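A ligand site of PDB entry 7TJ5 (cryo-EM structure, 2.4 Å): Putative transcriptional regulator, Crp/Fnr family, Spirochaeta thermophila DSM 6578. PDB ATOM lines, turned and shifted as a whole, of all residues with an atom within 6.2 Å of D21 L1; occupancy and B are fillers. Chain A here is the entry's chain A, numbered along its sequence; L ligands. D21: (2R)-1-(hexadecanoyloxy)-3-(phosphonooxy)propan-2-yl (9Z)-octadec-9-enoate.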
ATOM      1  N   ILE A  49     -24.018   4.089  22.730  1.00  0.00           N
ATOM      2  CA  ILE A  49     -25.155   4.865  22.198  1.00  0.00           C
ATOM      3  C   ILE A  49     -25.120   5.037  20.683  1.00  0.00           C
ATOM      4  O   ILE A  49     -26.120   4.678  20.032  1.00  0.00           O
ATOM      5  CB  ILE A  49     -25.281   6.231  22.916  1.00  0.00           C
ATOM      6  CG1 ILE A  49     -25.678   6.041  24.375  1.00  0.00           C
ATOM      7  CG2 ILE A  49     -26.291   7.112  22.202  1.00  0.00           C
ATOM      8  CD1 ILE A  49     -25.569   7.297  25.202  1.00  0.00           C
ATOM      9  N   PRO A  50     -24.064   5.568  20.053  1.00  0.00           N
ATOM     10  CA  PRO A  50     -24.107   5.666  18.578  1.00  0.00           C
ATOM     11  C   PRO A  50     -24.157   4.300  17.903  1.00  0.00           C
ATOM     12  O   PRO A  50     -24.794   4.152  16.848  1.00  0.00           O
ATOM     13  CB  PRO A  50     -22.823   6.422  18.232  1.00  0.00           C
ATOM     14  CG  PRO A  50     -21.931   6.212  19.389  1.00  0.00           C
ATOM     15  CD  PRO A  50     -22.827   6.172  20.577  1.00  0.00           C
ATOM     16  N   LEU A  53     -27.596   3.158  18.046  1.00  0.00           N
ATOM     17  CA  LEU A  53     -28.367   3.993  17.118  1.00  0.00           C
ATOM     18  C   LEU A  53     -28.252   3.458  15.707  1.00  0.00           C
ATOM     19  O   LEU A  53     -29.245   3.418  14.968  1.00  0.00           O
ATOM     20  CB  LEU A  53     -27.887   5.444  17.199  1.00  0.00           C
ATOM     21  CG  LEU A  53     -28.525   6.311  18.277  1.00  0.00           C
ATOM     22  CD1 LEU A  53     -27.914   7.701  18.275  1.00  0.00           C
ATOM     23  CD2 LEU A  53     -30.033   6.383  18.088  1.00  0.00           C
ATOM     24  N   VAL A  54     -27.050   3.061  15.294  1.00  0.00           N
ATOM     25  CA  VAL A  54     -26.872   2.457  13.974  1.00  0.00           C
ATOM     26  C   VAL A  54     -27.509   1.068  13.934  1.00  0.00           C
ATOM     27  O   VAL A  54     -28.219   0.712  12.993  1.00  0.00           O
ATOM     28  CB  VAL A  54     -25.391   2.408  13.590  1.00  0.00           C
ATOM     29  CG1 VAL A  54     -25.199   1.654  12.285  1.00  0.00           C
ATOM     30  CG2 VAL A  54     -24.836   3.816  13.493  1.00  0.00           C
ATOM     31  N   PRO A 120     -38.705   7.329  15.647  1.00  0.00           N
ATOM     32  CA  PRO A 120     -38.112   7.570  14.340  1.00  0.00           C
ATOM     33  C   PRO A 120     -36.791   8.322  14.454  1.00  0.00           C
ATOM     34  O   PRO A 120     -36.387   8.762  15.528  1.00  0.00           O
ATOM     35  CB  PRO A 120     -39.173   8.398  13.609  1.00  0.00           C
ATOM     36  CG  PRO A 120     -39.850   9.142  14.694  1.00  0.00           C
ATOM     37  CD  PRO A 120     -39.886   8.181  15.861  1.00  0.00           C
ATOM     38  N   SER A 121     -36.126   8.477  13.314  1.00  0.00           N
ATOM     39  CA  SER A 121     -34.785   9.066  13.300  1.00  0.00           C
ATOM     40  C   SER A 121     -34.720  10.478  13.879  1.00  0.00           C
ATOM     41  O   SER A 121     -33.754  10.755  14.610  1.00  0.00           O
ATOM     42  CB  SER A 121     -34.222   9.044  11.874  1.00  0.00           C
ATOM     43  OG  SER A 121     -34.244   7.735  11.330  1.00  0.00           O
ATOM     44  N   SER A 124     -34.910  10.082  17.655  1.00  0.00           N
ATOM     45  CA  SER A 124     -34.087   9.035  18.222  1.00  0.00           C
ATOM     46  C   SER A 124     -32.726   9.564  18.664  1.00  0.00           C
ATOM     47  O   SER A 124     -31.996   8.843  19.362  1.00  0.00           O
ATOM     48  CB  SER A 124     -33.884   7.891  17.227  1.00  0.00           C
ATOM     49  OG  SER A 124     -33.027   8.278  16.168  1.00  0.00           O
ATOM     50  N   LEU A 125     -32.377  10.791  18.278  1.00  0.00           N
ATOM     51  CA  LEU A 125     -31.076  11.359  18.569  1.00  0.00           C
ATOM     52  C   LEU A 125     -31.072  12.100  19.900  1.00  0.00           C
ATOM     53  O   LEU A 125     -30.186  12.922  20.152  1.00  0.00           O
ATOM     54  CB  LEU A 125     -30.636  12.312  17.447  1.00  0.00           C
ATOM     55  CG  LEU A 125     -30.507  11.713  16.051  1.00  0.00           C
ATOM     56  CD1 LEU A 125     -30.434  12.817  15.000  1.00  0.00           C
ATOM     57  CD2 LEU A 125     -29.285  10.810  15.966  1.00  0.00           C
ATOM     58  N   LEU A 128     -28.287  10.991  23.000  1.00  0.00           N
ATOM     59  CA  LEU A 128     -26.923  11.487  23.021  1.00  0.00           C
ATOM     60  C   LEU A 128     -26.741  12.642  23.985  1.00  0.00           C
ATOM     61  O   LEU A 128     -25.621  13.118  24.164  1.00  0.00           O
ATOM     62  CB  LEU A 128     -26.505  11.934  21.610  1.00  0.00           C
ATOM     63  CG  LEU A 128     -26.434  10.855  20.533  1.00  0.00           C
ATOM     64  CD1 LEU A 128     -26.715  11.465  19.168  1.00  0.00           C
ATOM     65  CD2 LEU A 128     -25.074  10.186  20.539  1.00  0.00           C
ATOM     66  N   ALA A 166     -15.085  11.172  19.113  1.00  0.00           N
ATOM     67  CA  ALA A 166     -15.774  11.840  18.019  1.00  0.00           C
ATOM     68  C   ALA A 166     -15.609  11.099  16.702  1.00  0.00           C
ATOM     69  O   ALA A 166     -16.527  11.088  15.891  1.00  0.00           O
ATOM     70  CB  ALA A 166     -15.262  13.278  17.890  1.00  0.00           C
ATOM     71  N   GLY A 169     -18.109   8.331  16.793  1.00  0.00           N
ATOM     72  CA  GLY A 169     -19.436   8.863  16.527  1.00  0.00           C
ATOM     73  C   GLY A 169     -19.643   9.257  15.077  1.00  0.00           C
ATOM     74  O   GLY A 169     -20.706   9.028  14.503  1.00  0.00           O
ATOM     75  N   ILE A 170     -18.615   9.841  14.459  1.00  0.00           N
ATOM     76  CA  ILE A 170     -18.703  10.259  13.069  1.00  0.00           C
ATOM     77  C   ILE A 170     -18.758   9.037  12.150  1.00  0.00           C
ATOM     78  O   ILE A 170     -19.474   9.037  11.139  1.00  0.00           O
ATOM     79  CB  ILE A 170     -17.523  11.188  12.720  1.00  0.00           C
ATOM     80  CG1 ILE A 170     -17.728  12.567  13.358  1.00  0.00           C
ATOM     81  CG2 ILE A 170     -17.362  11.342  11.213  1.00  0.00           C
ATOM     82  CD1 ILE A 170     -16.464  13.387  13.459  1.00  0.00           C
ATOM     83  N   CYS A 172     -20.109   6.188  13.013  1.00  0.00           N
ATOM     84  CA  CYS A 172     -21.487   5.705  13.151  1.00  0.00           C
ATOM     85  C   CYS A 172     -22.455   6.555  12.318  1.00  0.00           C
ATOM     86  O   CYS A 172     -23.338   6.010  11.647  1.00  0.00           O
ATOM     87  CB  CYS A 172     -21.893   5.717  14.619  1.00  0.00           C
ATOM     88  SG  CYS A 172     -21.185   4.372  15.594  1.00  0.00           S
ATOM     89  N   GLY A 173     -22.279   7.878  12.345  1.00  0.00           N
ATOM     90  CA  GLY A 173     -23.129   8.739  11.529  1.00  0.00           C
ATOM     91  C   GLY A 173     -22.970   8.504  10.041  1.00  0.00           C
ATOM     92  O   GLY A 173     -23.932   8.576   9.281  1.00  0.00           O
ATOM     93  N   TRP A 174     -21.736   8.218   9.607  1.00  0.00           N
ATOM     94  CA  TRP A 174     -21.501   7.900   8.200  1.00  0.00           C
ATOM     95  C   TRP A 174     -22.128   6.564   7.831  1.00  0.00           C
ATOM     96  O   TRP A 174     -22.671   6.411   6.721  1.00  0.00           O
ATOM     97  CB  TRP A 174     -19.992   7.887   7.925  1.00  0.00           C
ATOM     98  CG  TRP A 174     -19.605   7.370   6.573  1.00  0.00           C
ATOM     99  CD1 TRP A 174     -19.253   6.097   6.242  1.00  0.00           C
ATOM    100  CD2 TRP A 174     -19.529   8.131   5.352  1.00  0.00           C
ATOM    101  NE1 TRP A 174     -18.960   6.015   4.909  1.00  0.00           N
ATOM    102  CE2 TRP A 174     -19.117   7.248   4.340  1.00  0.00           C
ATOM    103  CE3 TRP A 174     -19.756   9.472   5.030  1.00  0.00           C
ATOM    104  CZ2 TRP A 174     -18.943   7.663   3.016  1.00  0.00           C
ATOM    105  CZ3 TRP A 174     -19.584   9.880   3.727  1.00  0.00           C
ATOM    106  CH2 TRP A 174     -19.181   8.977   2.734  1.00  0.00           C
ATOM    107  N   MET A 175     -22.066   5.576   8.729  1.00  0.00           N
ATOM    108  CA  MET A 175     -22.722   4.295   8.479  1.00  0.00           C
ATOM    109  C   MET A 175     -24.226   4.448   8.374  1.00  0.00           C
ATOM    110  O   MET A 175     -24.878   3.761   7.568  1.00  0.00           O
ATOM    111  CB  MET A 175     -22.379   3.296   9.576  1.00  0.00           C
ATOM    112  CG  MET A 175     -21.357   2.249   9.183  1.00  0.00           C
ATOM    113  SD  MET A 175     -21.061   1.070  10.524  1.00  0.00           S
ATOM    114  CE  MET A 175     -21.013   2.173  11.931  1.00  0.00           C
ATOM    115  N   SER A 176     -24.819   5.314   9.202  1.00  0.00           N
ATOM    116  CA  SER A 176     -26.277   5.452   9.208  1.00  0.00           C
ATOM    117  C   SER A 176     -26.795   5.967   7.867  1.00  0.00           C
ATOM    118  O   SER A 176     -27.779   5.441   7.337  1.00  0.00           O
ATOM    119  CB  SER A 176     -26.706   6.393  10.333  1.00  0.00           C
ATOM    120  OG  SER A 176     -26.933   7.697   9.837  1.00  0.00           O
ATOM    121  N   LEU A 177     -26.134   6.973   7.300  1.00  0.00           N
ATOM    122  CA  LEU A 177     -26.562   7.565   6.032  1.00  0.00           C
ATOM    123  C   LEU A 177     -25.850   6.954   4.828  1.00  0.00           C
ATOM    124  O   LEU A 177     -25.371   7.635   3.924  1.00  0.00           O
ATOM    125  CB  LEU A 177     -26.396   9.080   6.131  1.00  0.00           C
ATOM    126  CG  LEU A 177     -25.078   9.861   6.304  1.00  0.00           C
ATOM    127  CD1 LEU A 177     -24.369  10.280   5.034  1.00  0.00           C
ATOM    128  CD2 LEU A 177     -25.298  11.073   7.214  1.00  0.00           C
ATOM    129  N   GLN A 178     -25.855   5.617   4.771  1.00  0.00           N
ATOM    130  CA  GLN A 178     -25.350   4.802   3.675  1.00  0.00           C
ATOM    131  C   GLN A 178     -26.484   3.993   3.058  1.00  0.00           C
ATOM    132  O   GLN A 178     -27.475   3.696   3.733  1.00  0.00           O
ATOM    133  CB  GLN A 178     -24.253   3.843   4.152  1.00  0.00           C
ATOM    134  CG  GLN A 178     -22.855   4.448   4.194  1.00  0.00           C
ATOM    135  CD  GLN A 178     -22.288   4.738   2.821  1.00  0.00           C
ATOM    136  OE1 GLN A 178     -22.081   5.900   2.457  1.00  0.00           O
ATOM    137  NE2 GLN A 178     -22.038   3.693   2.051  1.00  0.00           N
ATOM    138  N   TYR A 218     -22.880  16.058   4.797  1.00  0.00           N
ATOM    139  CA  TYR A 218     -22.240  15.458   5.969  1.00  0.00           C
ATOM    140  C   TYR A 218     -20.717  15.493   5.839  1.00  0.00           C
ATOM    141  O   TYR A 218     -20.016  15.804   6.805  1.00  0.00           O
ATOM    142  CB  TYR A 218     -22.735  14.024   6.140  1.00  0.00           C
ATOM    143  CG  TYR A 218     -22.234  13.333   7.397  1.00  0.00           C
ATOM    144  CD1 TYR A 218     -22.696  13.719   8.642  1.00  0.00           C
ATOM    145  CD2 TYR A 218     -21.330  12.289   7.315  1.00  0.00           C
ATOM    146  CE1 TYR A 218     -22.241  13.089   9.792  1.00  0.00           C
ATOM    147  CE2 TYR A 218     -20.867  11.655   8.450  1.00  0.00           C
ATOM    148  CZ  TYR A 218     -21.332  12.060   9.683  1.00  0.00           C
ATOM    149  OH  TYR A 218     -20.890  11.428  10.826  1.00  0.00           O
ATOM    150  N   ILE A 222     -17.942  17.300   8.187  1.00  0.00           N
ATOM    151  CA  ILE A 222     -16.880  16.517   8.800  1.00  0.00           C
ATOM    152  C   ILE A 222     -15.506  17.041   8.389  1.00  0.00           C
ATOM    153  O   ILE A 222     -14.568  17.027   9.183  1.00  0.00           O
ATOM    154  CB  ILE A 222     -17.057  15.022   8.461  1.00  0.00           C
ATOM    155  CG1 ILE A 222     -18.342  14.480   9.101  1.00  0.00           C
ATOM    156  CG2 ILE A 222     -15.866  14.206   8.931  1.00  0.00           C
ATOM    157  CD1 ILE A 222     -18.496  14.841  10.557  1.00  0.00           C
ATOM    158  N   LEU A 225     -14.871  20.103  10.622  1.00  0.00           N
ATOM    159  CA  LEU A 225     -14.488  19.719  11.979  1.00  0.00           C
ATOM    160  C   LEU A 225     -13.127  19.024  12.018  1.00  0.00           C
ATOM    161  O   LEU A 225     -12.398  19.169  12.991  1.00  0.00           O
ATOM    162  CB  LEU A 225     -15.540  18.835  12.638  1.00  0.00           C
ATOM    163  CG  LEU A 225     -17.033  19.038  12.367  1.00  0.00           C
ATOM    164  CD1 LEU A 225     -17.846  17.887  12.930  1.00  0.00           C
ATOM    165  CD2 LEU A 225     -17.505  20.366  12.942  1.00  0.00           C
HETATM  166  C05 D21 L   1     -20.847  13.637  15.624  1.00  0.00           C
HETATM  167  C06 D21 L   1     -21.973  12.603  15.379  1.00  0.00           C
HETATM  168  C07 D21 L   1     -22.666  12.142  16.687  1.00  0.00           C
HETATM  169  C08 D21 L   1     -23.002  10.654  16.676  1.00  0.00           C
HETATM  170  C09 D21 L   1     -24.164  10.339  15.717  1.00  0.00           C
HETATM  171  C10 D21 L   1     -24.984   9.124  16.182  1.00  0.00           C
HETATM  172  C11 D21 L   1     -25.330   8.167  15.021  1.00  0.00           C
HETATM  173  C12 D21 L   1     -26.730   8.452  14.440  1.00  0.00           C
HETATM  174  C13 D21 L   1     -27.385   7.180  13.885  1.00  0.00           C
HETATM  175  C14 D21 L   1     -28.766   7.467  13.253  1.00  0.00           C
HETATM  176  C15 D21 L   1     -29.454   6.182  12.791  1.00  0.00           C
HETATM  177  C16 D21 L   1     -30.943   6.403  12.465  1.00  0.00           C
HETATM  178  O17 D21 L   1     -31.783   5.796  13.051  1.00  0.00           O
HETATM  179  O18 D21 L   1     -31.304   7.326  11.476  1.00  0.00           O
HETATM  180  C19 D21 L   1     -31.268   6.818  10.162  1.00  0.00           C
HETATM  181  C20 D21 L   1     -30.840   7.941   9.210  1.00  0.00           C
HETATM  182  C21 D21 L   1     -30.440   7.364   7.832  1.00  0.00           C
HETATM  183  O22 D21 L   1     -30.600   5.949   7.868  1.00  0.00           O
HETATM  184  O30 D21 L   1     -29.756   8.638   9.763  1.00  0.00           O
HETATM  185  C31 D21 L   1     -30.060   9.980  10.112  1.00  0.00           C
HETATM  186  O32 D21 L   1     -30.870  10.594   9.495  1.00  0.00           O
HETATM  187  C33 D21 L   1     -29.293  10.674  11.304  1.00  0.00           C
HETATM  188  C34 D21 L   1     -28.181  11.692  10.824  1.00  0.00           C
HETATM  189  C35 D21 L   1     -26.721  11.156  11.098  1.00  0.00           C
HETATM  190  C36 D21 L   1     -25.673  12.312  11.285  1.00  0.00           C
HETATM  191  C37 D21 L   1     -26.296  13.594  11.927  1.00  0.00           C
HETATM  192  C38 D21 L   1     -26.260  13.559  13.478  1.00  0.00           C
HETATM  193  C39 D21 L   1     -25.564  14.815  14.079  1.00  0.00           C
HETATM  194  C40 D21 L   1     -25.631  14.753  15.618  1.00  0.00           C
HETATM  195  C41 D21 L   1     -25.719  15.286  16.829  1.00  0.00           C
HETATM  196  C34 D21 L   2     -30.861   8.080   2.775  1.00  0.00           C
HETATM  197  C35 D21 L   2     -31.421   8.825   4.046  1.00  0.00           C
HETATM  198  C36 D21 L   2     -30.909  10.315   4.134  1.00  0.00           C
HETATM  199  C37 D21 L   2     -31.545  11.079   5.332  1.00  0.00           C
HETATM  200  C38 D21 L   2     -30.463  11.584   6.332  1.00  0.00           C
HETATM  201  C39 D21 L   2     -30.546  13.113   6.593  1.00  0.00           C
HETATM  202  C40 D21 L   2     -29.130  13.648   6.855  1.00  0.00           C
HETATM  203  C41 D21 L   2     -28.251  14.533   7.319  1.00  0.00           C
HETATM  204  C42 D21 L   2     -26.839  15.063   7.574  1.00  0.00           C
HETATM  205  C43 D21 L   2     -26.784  16.549   7.208  1.00  0.00           C
HETATM  206  C44 D21 L   2     -25.671  17.315   7.950  1.00  0.00           C
HETATM  207  C45 D21 L   2     -25.424  16.782   9.380  1.00  0.00           C
HETATM  208  C46 D21 L   2     -24.314  17.589  10.118  1.00  0.00           C
HETATM  209  C47 D21 L   2     -23.997  16.999  11.520  1.00  0.00           C
HETATM  210  C48 D21 L   2     -23.460  18.076  12.497  1.00  0.00           C
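Merely in contact with D21 L1: Leu 53 (3.5 Å), Gly 169 (3.6 Å), Leu 125 (3.8 Å) and Tyr 218 (3.8 Å).
Hydrophobic or aromatic side chains that line D21 L1: Leu 53, Leu 125 and Tyr 218.
Of the 22 residues printed, 6 come within 4 Å of D21 L1.
The nearest printed residue that does not touch D21 L1 is Ile 170 (4.001 Å).
OG of Ser 176 lies within hydrogen-bond range of O30 of D21 L1, 3.0 Å away.
O18 of D21 L1 sits at hydrogen-bond distance from OG of Ser 121 (3.0 Å).
OH of Tyr 218 lies within hydrogen-bond range of O of Ile 170, 2.8 Å away.
The side-chain hydroxyl of Ser 124 is in hydrogen-bond range of the backbone carbonyl oxygen of Ser 121 (3.0 Å).
The side-chain hydroxyl (OG) of Ser 176 is in hydrogen-bond range of the backbone carbonyl oxygen (O) of Gly 173, 3.2 Å away.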
